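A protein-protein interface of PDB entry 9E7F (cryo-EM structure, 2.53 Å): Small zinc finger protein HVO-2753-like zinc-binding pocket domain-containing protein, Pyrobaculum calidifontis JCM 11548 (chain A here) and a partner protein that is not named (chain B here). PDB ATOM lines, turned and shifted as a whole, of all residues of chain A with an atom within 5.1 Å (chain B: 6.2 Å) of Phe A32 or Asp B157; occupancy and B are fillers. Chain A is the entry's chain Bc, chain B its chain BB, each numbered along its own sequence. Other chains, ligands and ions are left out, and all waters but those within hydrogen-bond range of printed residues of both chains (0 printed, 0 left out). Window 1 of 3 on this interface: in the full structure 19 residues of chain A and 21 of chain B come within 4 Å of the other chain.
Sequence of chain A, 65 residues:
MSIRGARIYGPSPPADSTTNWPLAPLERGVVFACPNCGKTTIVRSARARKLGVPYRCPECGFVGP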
ATOM      1  N   VAL A  30     -26.140 -16.239 -15.959  1.00  0.00           N
ATOM      2  CA  VAL A  30     -25.161 -15.192 -15.709  1.00  0.00           C
ATOM      3  C   VAL A  30     -25.850 -14.024 -15.023  1.00  0.00           C
ATOM      4  O   VAL A  30     -26.923 -13.585 -15.447  1.00  0.00           O
ATOM      5  CB  VAL A  30     -24.477 -14.744 -17.014  1.00  0.00           C
ATOM      6  CG1 VAL A  30     -23.910 -13.369 -16.855  1.00  0.00           C
ATOM      7  CG2 VAL A  30     -23.379 -15.711 -17.376  1.00  0.00           C
ATOM      8  N   VAL A  31     -25.226 -13.518 -13.963  1.00  0.00           N
ATOM      9  CA  VAL A  31     -25.773 -12.433 -13.161  1.00  0.00           C
ATOM     10  C   VAL A  31     -24.745 -11.316 -13.083  1.00  0.00           C
ATOM     11  O   VAL A  31     -23.556 -11.576 -12.878  1.00  0.00           O
ATOM     12  CB  VAL A  31     -26.154 -12.899 -11.745  1.00  0.00           C
ATOM     13  CG1 VAL A  31     -27.188 -11.968 -11.155  1.00  0.00           C
ATOM     14  CG2 VAL A  31     -26.660 -14.328 -11.771  1.00  0.00           C
ATOM     15  N   PHE A  32     -25.202 -10.080 -13.245  1.00  0.00           N
ATOM     16  CA  PHE A  32     -24.353  -8.913 -13.070  1.00  0.00           C
ATOM     17  C   PHE A  32     -25.258  -7.709 -12.836  1.00  0.00           C
ATOM     18  O   PHE A  32     -26.480  -7.844 -12.733  1.00  0.00           O
ATOM     19  CB  PHE A  32     -23.409  -8.725 -14.267  1.00  0.00           C
ATOM     20  CG  PHE A  32     -24.074  -8.853 -15.614  1.00  0.00           C
ATOM     21  CD1 PHE A  32     -24.169 -10.072 -16.250  1.00  0.00           C
ATOM     22  CD2 PHE A  32     -24.571  -7.740 -16.257  1.00  0.00           C
ATOM     23  CE1 PHE A  32     -24.770 -10.178 -17.481  1.00  0.00           C
ATOM     24  CE2 PHE A  32     -25.170  -7.840 -17.489  1.00  0.00           C
ATOM     25  CZ  PHE A  32     -25.270  -9.058 -18.103  1.00  0.00           C
ATOM     26  N   ALA A  33     -24.659  -6.531 -12.734  1.00  0.00           N
ATOM     27  CA  ALA A  33     -25.399  -5.292 -12.564  1.00  0.00           C
ATOM     28  C   ALA A  33     -25.602  -4.627 -13.916  1.00  0.00           C
ATOM     29  O   ALA A  33     -25.050  -5.063 -14.929  1.00  0.00           O
ATOM     30  CB  ALA A  33     -24.666  -4.344 -11.614  1.00  0.00           C
ATOM     31  N   CYS A  34     -26.409  -3.574 -13.930  1.00  0.00           N
ATOM     32  CA  CYS A  34     -26.635  -2.835 -15.160  1.00  0.00           C
ATOM     33  C   CYS A  34     -25.323  -2.215 -15.637  1.00  0.00           C
ATOM     34  O   CYS A  34     -24.584  -1.648 -14.822  1.00  0.00           O
ATOM     35  CB  CYS A  34     -27.682  -1.741 -14.960  1.00  0.00           C
ATOM     36  SG  CYS A  34     -27.847  -0.640 -16.386  1.00  0.00           S
ATOM     37  N   PRO A  35     -24.973  -2.360 -16.918  1.00  0.00           N
ATOM     38  CA  PRO A  35     -23.705  -1.789 -17.397  1.00  0.00           C
ATOM     39  C   PRO A  35     -23.632  -0.283 -17.257  1.00  0.00           C
ATOM     40  O   PRO A  35     -22.568   0.256 -16.932  1.00  0.00           O
ATOM     41  CB  PRO A  35     -23.662  -2.227 -18.867  1.00  0.00           C
ATOM     42  CG  PRO A  35     -24.614  -3.372 -18.955  1.00  0.00           C
ATOM     43  CD  PRO A  35     -25.701  -3.051 -17.991  1.00  0.00           C
ATOM     44  N   THR A  40     -29.278  -1.965 -10.697  1.00  0.00           N
ATOM     45  CA  THR A  40     -30.133  -3.136 -10.788  1.00  0.00           C
ATOM     46  C   THR A  40     -29.327  -4.344 -11.245  1.00  0.00           C
ATOM     47  O   THR A  40     -28.255  -4.222 -11.842  1.00  0.00           O
ATOM     48  CB  THR A  40     -31.296  -2.878 -11.742  1.00  0.00           C
ATOM     49  OG1 THR A  40     -31.690  -1.507 -11.638  1.00  0.00           O
ATOM     50  CG2 THR A  40     -32.481  -3.759 -11.389  1.00  0.00           C
ATOM     51  N   THR A  41     -29.860  -5.526 -10.956  1.00  0.00           N
ATOM     52  CA  THR A  41     -29.187  -6.783 -11.251  1.00  0.00           C
ATOM     53  C   THR A  41     -29.843  -7.455 -12.448  1.00  0.00           C
ATOM     54  O   THR A  41     -31.068  -7.598 -12.493  1.00  0.00           O
ATOM     55  CB  THR A  41     -29.217  -7.711 -10.041  1.00  0.00           C
ATOM     56  OG1 THR A  41     -28.578  -7.064  -8.937  1.00  0.00           O
ATOM     57  CG2 THR A  41     -28.489  -8.999 -10.346  1.00  0.00           C
ATOM     58  N   ILE A  42     -29.025  -7.872 -13.407  1.00  0.00           N
ATOM     59  CA  ILE A  42     -29.493  -8.473 -14.647  1.00  0.00           C
ATOM     60  C   ILE A  42     -29.204  -9.964 -14.594  1.00  0.00           C
ATOM     61  O   ILE A  42     -28.046 -10.374 -14.456  1.00  0.00           O
ATOM     62  CB  ILE A  42     -28.828  -7.831 -15.870  1.00  0.00           C
ATOM     63  CG1 ILE A  42     -29.390  -6.430 -16.096  1.00  0.00           C
ATOM     64  CG2 ILE A  42     -29.056  -8.683 -17.097  1.00  0.00           C
ATOM     65  CD1 ILE A  42     -30.898  -6.384 -16.157  1.00  0.00           C
ATOM     66  N   ARG A  44     -29.554 -13.458 -16.716  1.00  0.00           N
ATOM     67  CA  ARG A  44     -29.713 -13.979 -18.068  1.00  0.00           C
ATOM     68  C   ARG A  44     -29.560 -15.490 -18.027  1.00  0.00           C
ATOM     69  O   ARG A  44     -28.468 -15.998 -17.764  1.00  0.00           O
ATOM     70  CB  ARG A  44     -28.694 -13.358 -19.019  1.00  0.00           C
ATOM     71  CG  ARG A  44     -29.270 -12.310 -19.934  1.00  0.00           C
ATOM     72  CD  ARG A  44     -28.197 -11.396 -20.478  1.00  0.00           C
ATOM     73  NE  ARG A  44     -27.629 -11.866 -21.736  1.00  0.00           N
ATOM     74  CZ  ARG A  44     -28.267 -11.865 -22.899  1.00  0.00           C
ATOM     75  NH1 ARG A  44     -29.520 -11.463 -23.001  1.00  0.00           N
ATOM     76  NH2 ARG A  44     -27.626 -12.273 -23.988  1.00  0.00           N
ATOM     77  N   ARG A  49     -29.076 -16.117 -23.378  1.00  0.00           N
ATOM     78  CA  ARG A  49     -27.746 -15.778 -23.871  1.00  0.00           C
ATOM     79  C   ARG A  49     -27.512 -16.346 -25.259  1.00  0.00           C
ATOM     80  O   ARG A  49     -26.913 -15.685 -26.113  1.00  0.00           O
ATOM     81  CB  ARG A  49     -26.678 -16.277 -22.900  1.00  0.00           C
ATOM     82  CG  ARG A  49     -26.931 -15.883 -21.463  1.00  0.00           C
ATOM     83  CD  ARG A  49     -26.112 -16.700 -20.491  1.00  0.00           C
ATOM     84  NE  ARG A  49     -24.779 -17.015 -20.984  1.00  0.00           N
ATOM     85  CZ  ARG A  49     -23.746 -16.189 -20.915  1.00  0.00           C
ATOM     86  NH1 ARG A  49     -23.873 -14.973 -20.425  1.00  0.00           N
ATOM     87  NH2 ARG A  49     -22.557 -16.597 -21.340  1.00  0.00           N
ATOM     88  N   TYR A  55     -32.274  -7.328 -22.929  1.00  0.00           N
ATOM     89  CA  TYR A  55     -32.654  -6.997 -21.566  1.00  0.00           C
ATOM     90  C   TYR A  55     -32.744  -5.486 -21.441  1.00  0.00           C
ATOM     91  O   TYR A  55     -32.159  -4.744 -22.231  1.00  0.00           O
ATOM     92  CB  TYR A  55     -31.652  -7.556 -20.547  1.00  0.00           C
ATOM     93  CG  TYR A  55     -30.210  -7.277 -20.901  1.00  0.00           C
ATOM     94  CD1 TYR A  55     -29.599  -6.085 -20.543  1.00  0.00           C
ATOM     95  CD2 TYR A  55     -29.462  -8.206 -21.601  1.00  0.00           C
ATOM     96  CE1 TYR A  55     -28.292  -5.830 -20.871  1.00  0.00           C
ATOM     97  CE2 TYR A  55     -28.155  -7.959 -21.931  1.00  0.00           C
ATOM     98  CZ  TYR A  55     -27.575  -6.773 -21.562  1.00  0.00           C
ATOM     99  OH  TYR A  55     -26.269  -6.527 -21.892  1.00  0.00           O
ATOM    100  N   GLY A  64     -29.598  -4.090 -23.689  1.00  0.00           N
ATOM    101  CA  GLY A  64     -28.419  -4.784 -24.138  1.00  0.00           C
ATOM    102  C   GLY A  64     -28.642  -5.499 -25.449  1.00  0.00           C
ATOM    103  O   GLY A  64     -29.531  -5.147 -26.227  1.00  0.00           O
ATOM    104  N   PRO A  65     -27.826  -6.528 -25.721  1.00  0.00           N
ATOM    105  CA  PRO A  65     -27.936  -7.344 -26.932  1.00  0.00           C
ATOM    106  C   PRO A  65     -29.298  -8.018 -27.055  1.00  0.00           C
ATOM    107  O   PRO A  65     -29.804  -8.143 -28.171  1.00  0.00           O
ATOM    108  CB  PRO A  65     -26.825  -8.384 -26.753  1.00  0.00           C
ATOM    109  CG  PRO A  65     -26.550  -8.407 -25.297  1.00  0.00           C
ATOM    110  CD  PRO A  65     -26.743  -7.000 -24.848  1.00  0.00           C
ATOM    111  N   LEU B  64     -18.453  -1.012 -16.895  1.00  0.00           N
ATOM    112  CA  LEU B  64     -18.660  -2.407 -16.529  1.00  0.00           C
ATOM    113  C   LEU B  64     -17.361  -3.045 -16.056  1.00  0.00           C
ATOM    114  O   LEU B  64     -17.342  -3.778 -15.061  1.00  0.00           O
ATOM    115  CB  LEU B  64     -19.251  -3.154 -17.730  1.00  0.00           C
ATOM    116  CG  LEU B  64     -19.705  -4.626 -17.766  1.00  0.00           C
ATOM    117  CD1 LEU B  64     -18.626  -5.667 -17.505  1.00  0.00           C
ATOM    118  CD2 LEU B  64     -20.871  -4.830 -16.819  1.00  0.00           C
ATOM    119  N   TYR B  68     -15.127  -4.663 -11.606  1.00  0.00           N
ATOM    120  CA  TYR B  68     -14.522  -5.923 -11.227  1.00  0.00           C
ATOM    121  C   TYR B  68     -13.077  -5.682 -10.820  1.00  0.00           C
ATOM    122  O   TYR B  68     -12.481  -4.684 -11.240  1.00  0.00           O
ATOM    123  CB  TYR B  68     -14.557  -6.979 -12.355  1.00  0.00           C
ATOM    124  CG  TYR B  68     -15.934  -7.326 -12.889  1.00  0.00           C
ATOM    125  CD1 TYR B  68     -16.637  -6.453 -13.708  1.00  0.00           C
ATOM    126  CD2 TYR B  68     -16.546  -8.521 -12.539  1.00  0.00           C
ATOM    127  CE1 TYR B  68     -17.888  -6.763 -14.172  1.00  0.00           C
ATOM    128  CE2 TYR B  68     -17.801  -8.838 -13.002  1.00  0.00           C
ATOM    129  CZ  TYR B  68     -18.464  -7.956 -13.816  1.00  0.00           C
ATOM    130  OH  TYR B  68     -19.716  -8.269 -14.278  1.00  0.00           O
ATOM    131  N   ILE B 141     -19.846 -17.288 -17.367  1.00  0.00           N
ATOM    132  CA  ILE B 141     -19.063 -16.077 -17.141  1.00  0.00           C
ATOM    133  C   ILE B 141     -19.511 -15.029 -18.147  1.00  0.00           C
ATOM    134  O   ILE B 141     -19.667 -15.351 -19.329  1.00  0.00           O
ATOM    135  CB  ILE B 141     -17.554 -16.344 -17.267  1.00  0.00           C
ATOM    136  CG1 ILE B 141     -17.075 -17.173 -16.080  1.00  0.00           C
ATOM    137  CG2 ILE B 141     -16.795 -15.042 -17.379  1.00  0.00           C
ATOM    138  CD1 ILE B 141     -16.540 -18.526 -16.450  1.00  0.00           C
ATOM    139  N   PRO B 142     -19.761 -13.792 -17.722  1.00  0.00           N
ATOM    140  CA  PRO B 142     -20.156 -12.743 -18.670  1.00  0.00           C
ATOM    141  C   PRO B 142     -19.075 -12.466 -19.702  1.00  0.00           C
ATOM    142  O   PRO B 142     -17.885 -12.648 -19.451  1.00  0.00           O
ATOM    143  CB  PRO B 142     -20.394 -11.520 -17.779  1.00  0.00           C
ATOM    144  CG  PRO B 142     -20.263 -11.978 -16.378  1.00  0.00           C
ATOM    145  CD  PRO B 142     -20.078 -13.444 -16.332  1.00  0.00           C
ATOM    146  N   VAL B 143     -19.509 -12.032 -20.883  1.00  0.00           N
ATOM    147  CA  VAL B 143     -18.628 -11.835 -22.025  1.00  0.00           C
ATOM    148  C   VAL B 143     -18.875 -10.462 -22.629  1.00  0.00           C
ATOM    149  O   VAL B 143     -20.021 -10.017 -22.737  1.00  0.00           O
ATOM    150  CB  VAL B 143     -18.832 -12.927 -23.092  1.00  0.00           C
ATOM    151  CG1 VAL B 143     -17.919 -12.687 -24.279  1.00  0.00           C
ATOM    152  CG2 VAL B 143     -18.589 -14.290 -22.497  1.00  0.00           C
ATOM    153  N   VAL B 144     -17.797  -9.795 -23.023  1.00  0.00           N
ATOM    154  CA  VAL B 144     -17.851  -8.581 -23.823  1.00  0.00           C
ATOM    155  C   VAL B 144     -17.036  -8.822 -25.081  1.00  0.00           C
ATOM    156  O   VAL B 144     -16.080  -9.602 -25.073  1.00  0.00           O
ATOM    157  CB  VAL B 144     -17.313  -7.362 -23.052  1.00  0.00           C
ATOM    158  CG1 VAL B 144     -17.714  -6.076 -23.748  1.00  0.00           C
ATOM    159  CG2 VAL B 144     -17.798  -7.395 -21.615  1.00  0.00           C
ATOM    160  N   TYR B 155     -24.202 -15.672 -26.819  1.00  0.00           N
ATOM    161  CA  TYR B 155     -23.552 -15.650 -25.515  1.00  0.00           C
ATOM    162  C   TYR B 155     -22.719 -14.397 -25.292  1.00  0.00           C
ATOM    163  O   TYR B 155     -21.719 -14.437 -24.578  1.00  0.00           O
ATOM    164  CB  TYR B 155     -22.673 -16.882 -25.322  1.00  0.00           C
ATOM    165  CG  TYR B 155     -23.380 -18.181 -25.545  1.00  0.00           C
ATOM    166  CD1 TYR B 155     -24.374 -18.605 -24.686  1.00  0.00           C
ATOM    167  CD2 TYR B 155     -23.049 -18.993 -26.614  1.00  0.00           C
ATOM    168  CE1 TYR B 155     -25.016 -19.796 -24.880  1.00  0.00           C
ATOM    169  CE2 TYR B 155     -23.687 -20.186 -26.817  1.00  0.00           C
ATOM    170  CZ  TYR B 155     -24.671 -20.583 -25.947  1.00  0.00           C
ATOM    171  OH  TYR B 155     -25.318 -21.776 -26.146  1.00  0.00           O
ATOM    172  N   ILE B 156     -23.103 -13.281 -25.886  1.00  0.00           N
ATOM    173  CA  ILE B 156     -22.392 -12.023 -25.714  1.00  0.00           C
ATOM    174  C   ILE B 156     -23.302 -11.107 -24.910  1.00  0.00           C
ATOM    175  O   ILE B 156     -24.262 -10.542 -25.442  1.00  0.00           O
ATOM    176  CB  ILE B 156     -22.001 -11.396 -27.053  1.00  0.00           C
ATOM    177  CG1 ILE B 156     -21.343 -12.444 -27.939  1.00  0.00           C
ATOM    178  CG2 ILE B 156     -21.055 -10.247 -26.833  1.00  0.00           C
ATOM    179  CD1 ILE B 156     -19.866 -12.501 -27.796  1.00  0.00           C
ATOM    180  N   ASP B 157     -22.999 -10.954 -23.622  1.00  0.00           N
ATOM    181  CA  ASP B 157     -23.839 -10.144 -22.753  1.00  0.00           C
ATOM    182  C   ASP B 157     -23.680  -8.656 -23.007  1.00  0.00           C
ATOM    183  O   ASP B 157     -24.637  -7.904 -22.813  1.00  0.00           O
ATOM    184  CB  ASP B 157     -23.529 -10.467 -21.301  1.00  0.00           C
ATOM    185  CG  ASP B 157     -23.448 -11.945 -21.058  1.00  0.00           C
ATOM    186  OD1 ASP B 157     -24.448 -12.642 -21.308  1.00  0.00           O
ATOM    187  OD2 ASP B 157     -22.384 -12.427 -20.637  1.00  0.00           O
ATOM    188  N   PHE B 158     -22.502  -8.213 -23.430  1.00  0.00           N
ATOM    189  CA  PHE B 158     -22.314  -6.837 -23.854  1.00  0.00           C
ATOM    190  C   PHE B 158     -21.515  -6.827 -25.145  1.00  0.00           C
ATOM    191  O   PHE B 158     -20.505  -7.522 -25.259  1.00  0.00           O
ATOM    192  CB  PHE B 158     -21.597  -6.009 -22.789  1.00  0.00           C
ATOM    193  CG  PHE B 158     -21.656  -4.535 -23.039  1.00  0.00           C
ATOM    194  CD1 PHE B 158     -22.743  -3.796 -22.625  1.00  0.00           C
ATOM    195  CD2 PHE B 158     -20.635  -3.890 -23.706  1.00  0.00           C
ATOM    196  CE1 PHE B 158     -22.802  -2.442 -22.860  1.00  0.00           C
ATOM    197  CE2 PHE B 158     -20.694  -2.535 -23.944  1.00  0.00           C
ATOM    198  CZ  PHE B 158     -21.779  -1.814 -23.519  1.00  0.00           C
ATOM    199  N   MET B 159     -21.966  -6.038 -26.113  1.00  0.00           N
ATOM    200  CA  MET B 159     -21.300  -5.948 -27.399  1.00  0.00           C
ATOM    201  C   MET B 159     -20.992  -4.498 -27.729  1.00  0.00           C
ATOM    202  O   MET B 159     -21.707  -3.584 -27.316  1.00  0.00           O
ATOM    203  CB  MET B 159     -22.146  -6.550 -28.523  1.00  0.00           C
ATOM    204  CG  MET B 159     -23.172  -5.599 -29.104  1.00  0.00           C
ATOM    205  SD  MET B 159     -24.357  -6.452 -30.155  1.00  0.00           S
ATOM    206  CE  MET B 159     -24.469  -8.026 -29.319  1.00  0.00           C
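Among the printed residues, pairs that only touch across the chains: Pro A65 with Asp B157, Pro A65 with Ile B156, Pro A65 with Met B159, Phe A32 with Tyr B68, Arg A49 with Ile B141, Val A30 with Pro B142, Val A30 with Ile B141 and Phe A32 with Asp B157.
Phe A32 touches just these residues of chain B: Tyr B68 and Asp B157.
Of chain A, only Phe A32 (3.9 Å), Arg A44 (3.3 Å), Arg A49 (2.6 Å), Tyr A55 (2.3 Å) and Pro A65 (3.1 Å) come within 4 Å of Asp B157.
Of the printed residues of chain A, Tyr B68 touches Phe A32 (3.7 Å).
Of the printed residues of chain A, Tyr B155 touches Arg A49.
Val A31 touches none of the printed residues of chain B.
The nearest residue of chain A that does not touch Asp B157 is Val A30 (4.2 Å).
The backbone carbonyl oxygen (O) of Arg A49 sits at hydrogen-bond distance from the backbone NH (N) of Tyr B155, at 2.8 Å.
The guanidinium group (NE) of Arg A44 lies within salt-bridge range of the side-chain carboxylate (OD1) of Asp B157, at 3.3 Å.
OD1 of Asp B157 is in salt-bridge range of NH1 of Arg A49 (2.6 Å).
The side-chain hydroxyl (OH) of Tyr A55 sits close to the backbone carbonyl oxygen (O) of Asp B157.
The backbone NH (N) of Val B143 is in hydrogen-bond range of the side-chain carboxylate (OD2) of Asp B157 (2.9 Å).
The backbone NH (N) of Arg A44 lies within hydrogen-bond range of the backbone carbonyl oxygen (O) of Val A30 (2.9 Å).
The backbone carbonyl oxygen (O) of Phe A32 is in hydrogen-bond range of the backbone NH (N) of Ile A42.
The backbone NH (N) of Gly A64 lies within hydrogen-bond range of the backbone carbonyl oxygen (O) of Tyr A55.
Of the 14 printed residues of chain A, 6 touch a printed residue of chain B.
Printed residues of chain A that touch a printed residue of chain B: Val A30, Phe A32, Arg A44, Arg A49, Tyr A55 and Pro A65.
Of the 11 printed residues of chain B, 7 touch a printed residue of chain A.
Printed residues of chain B that touch a printed residue of chain A: Tyr B68, Ile B141, Pro B142, Tyr B155, Ile B156, Asp B157 and Met B159.
Hydrophobic or aromatic side chains of chain B within 4 Å of the printed part of chain A: Tyr B68, Pro B142, Tyr B155 and Met B159.
Among the printed residues, 12 pairs touch across the chains.
Among the printed residues, Asp or Glu carboxylates within 4 Å of a Lys or Arg side-chain nitrogen of the other chain: Arg A44 with Asp B157 (3.3 Å) and Arg A49 with Asp B157 (2.6 Å).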
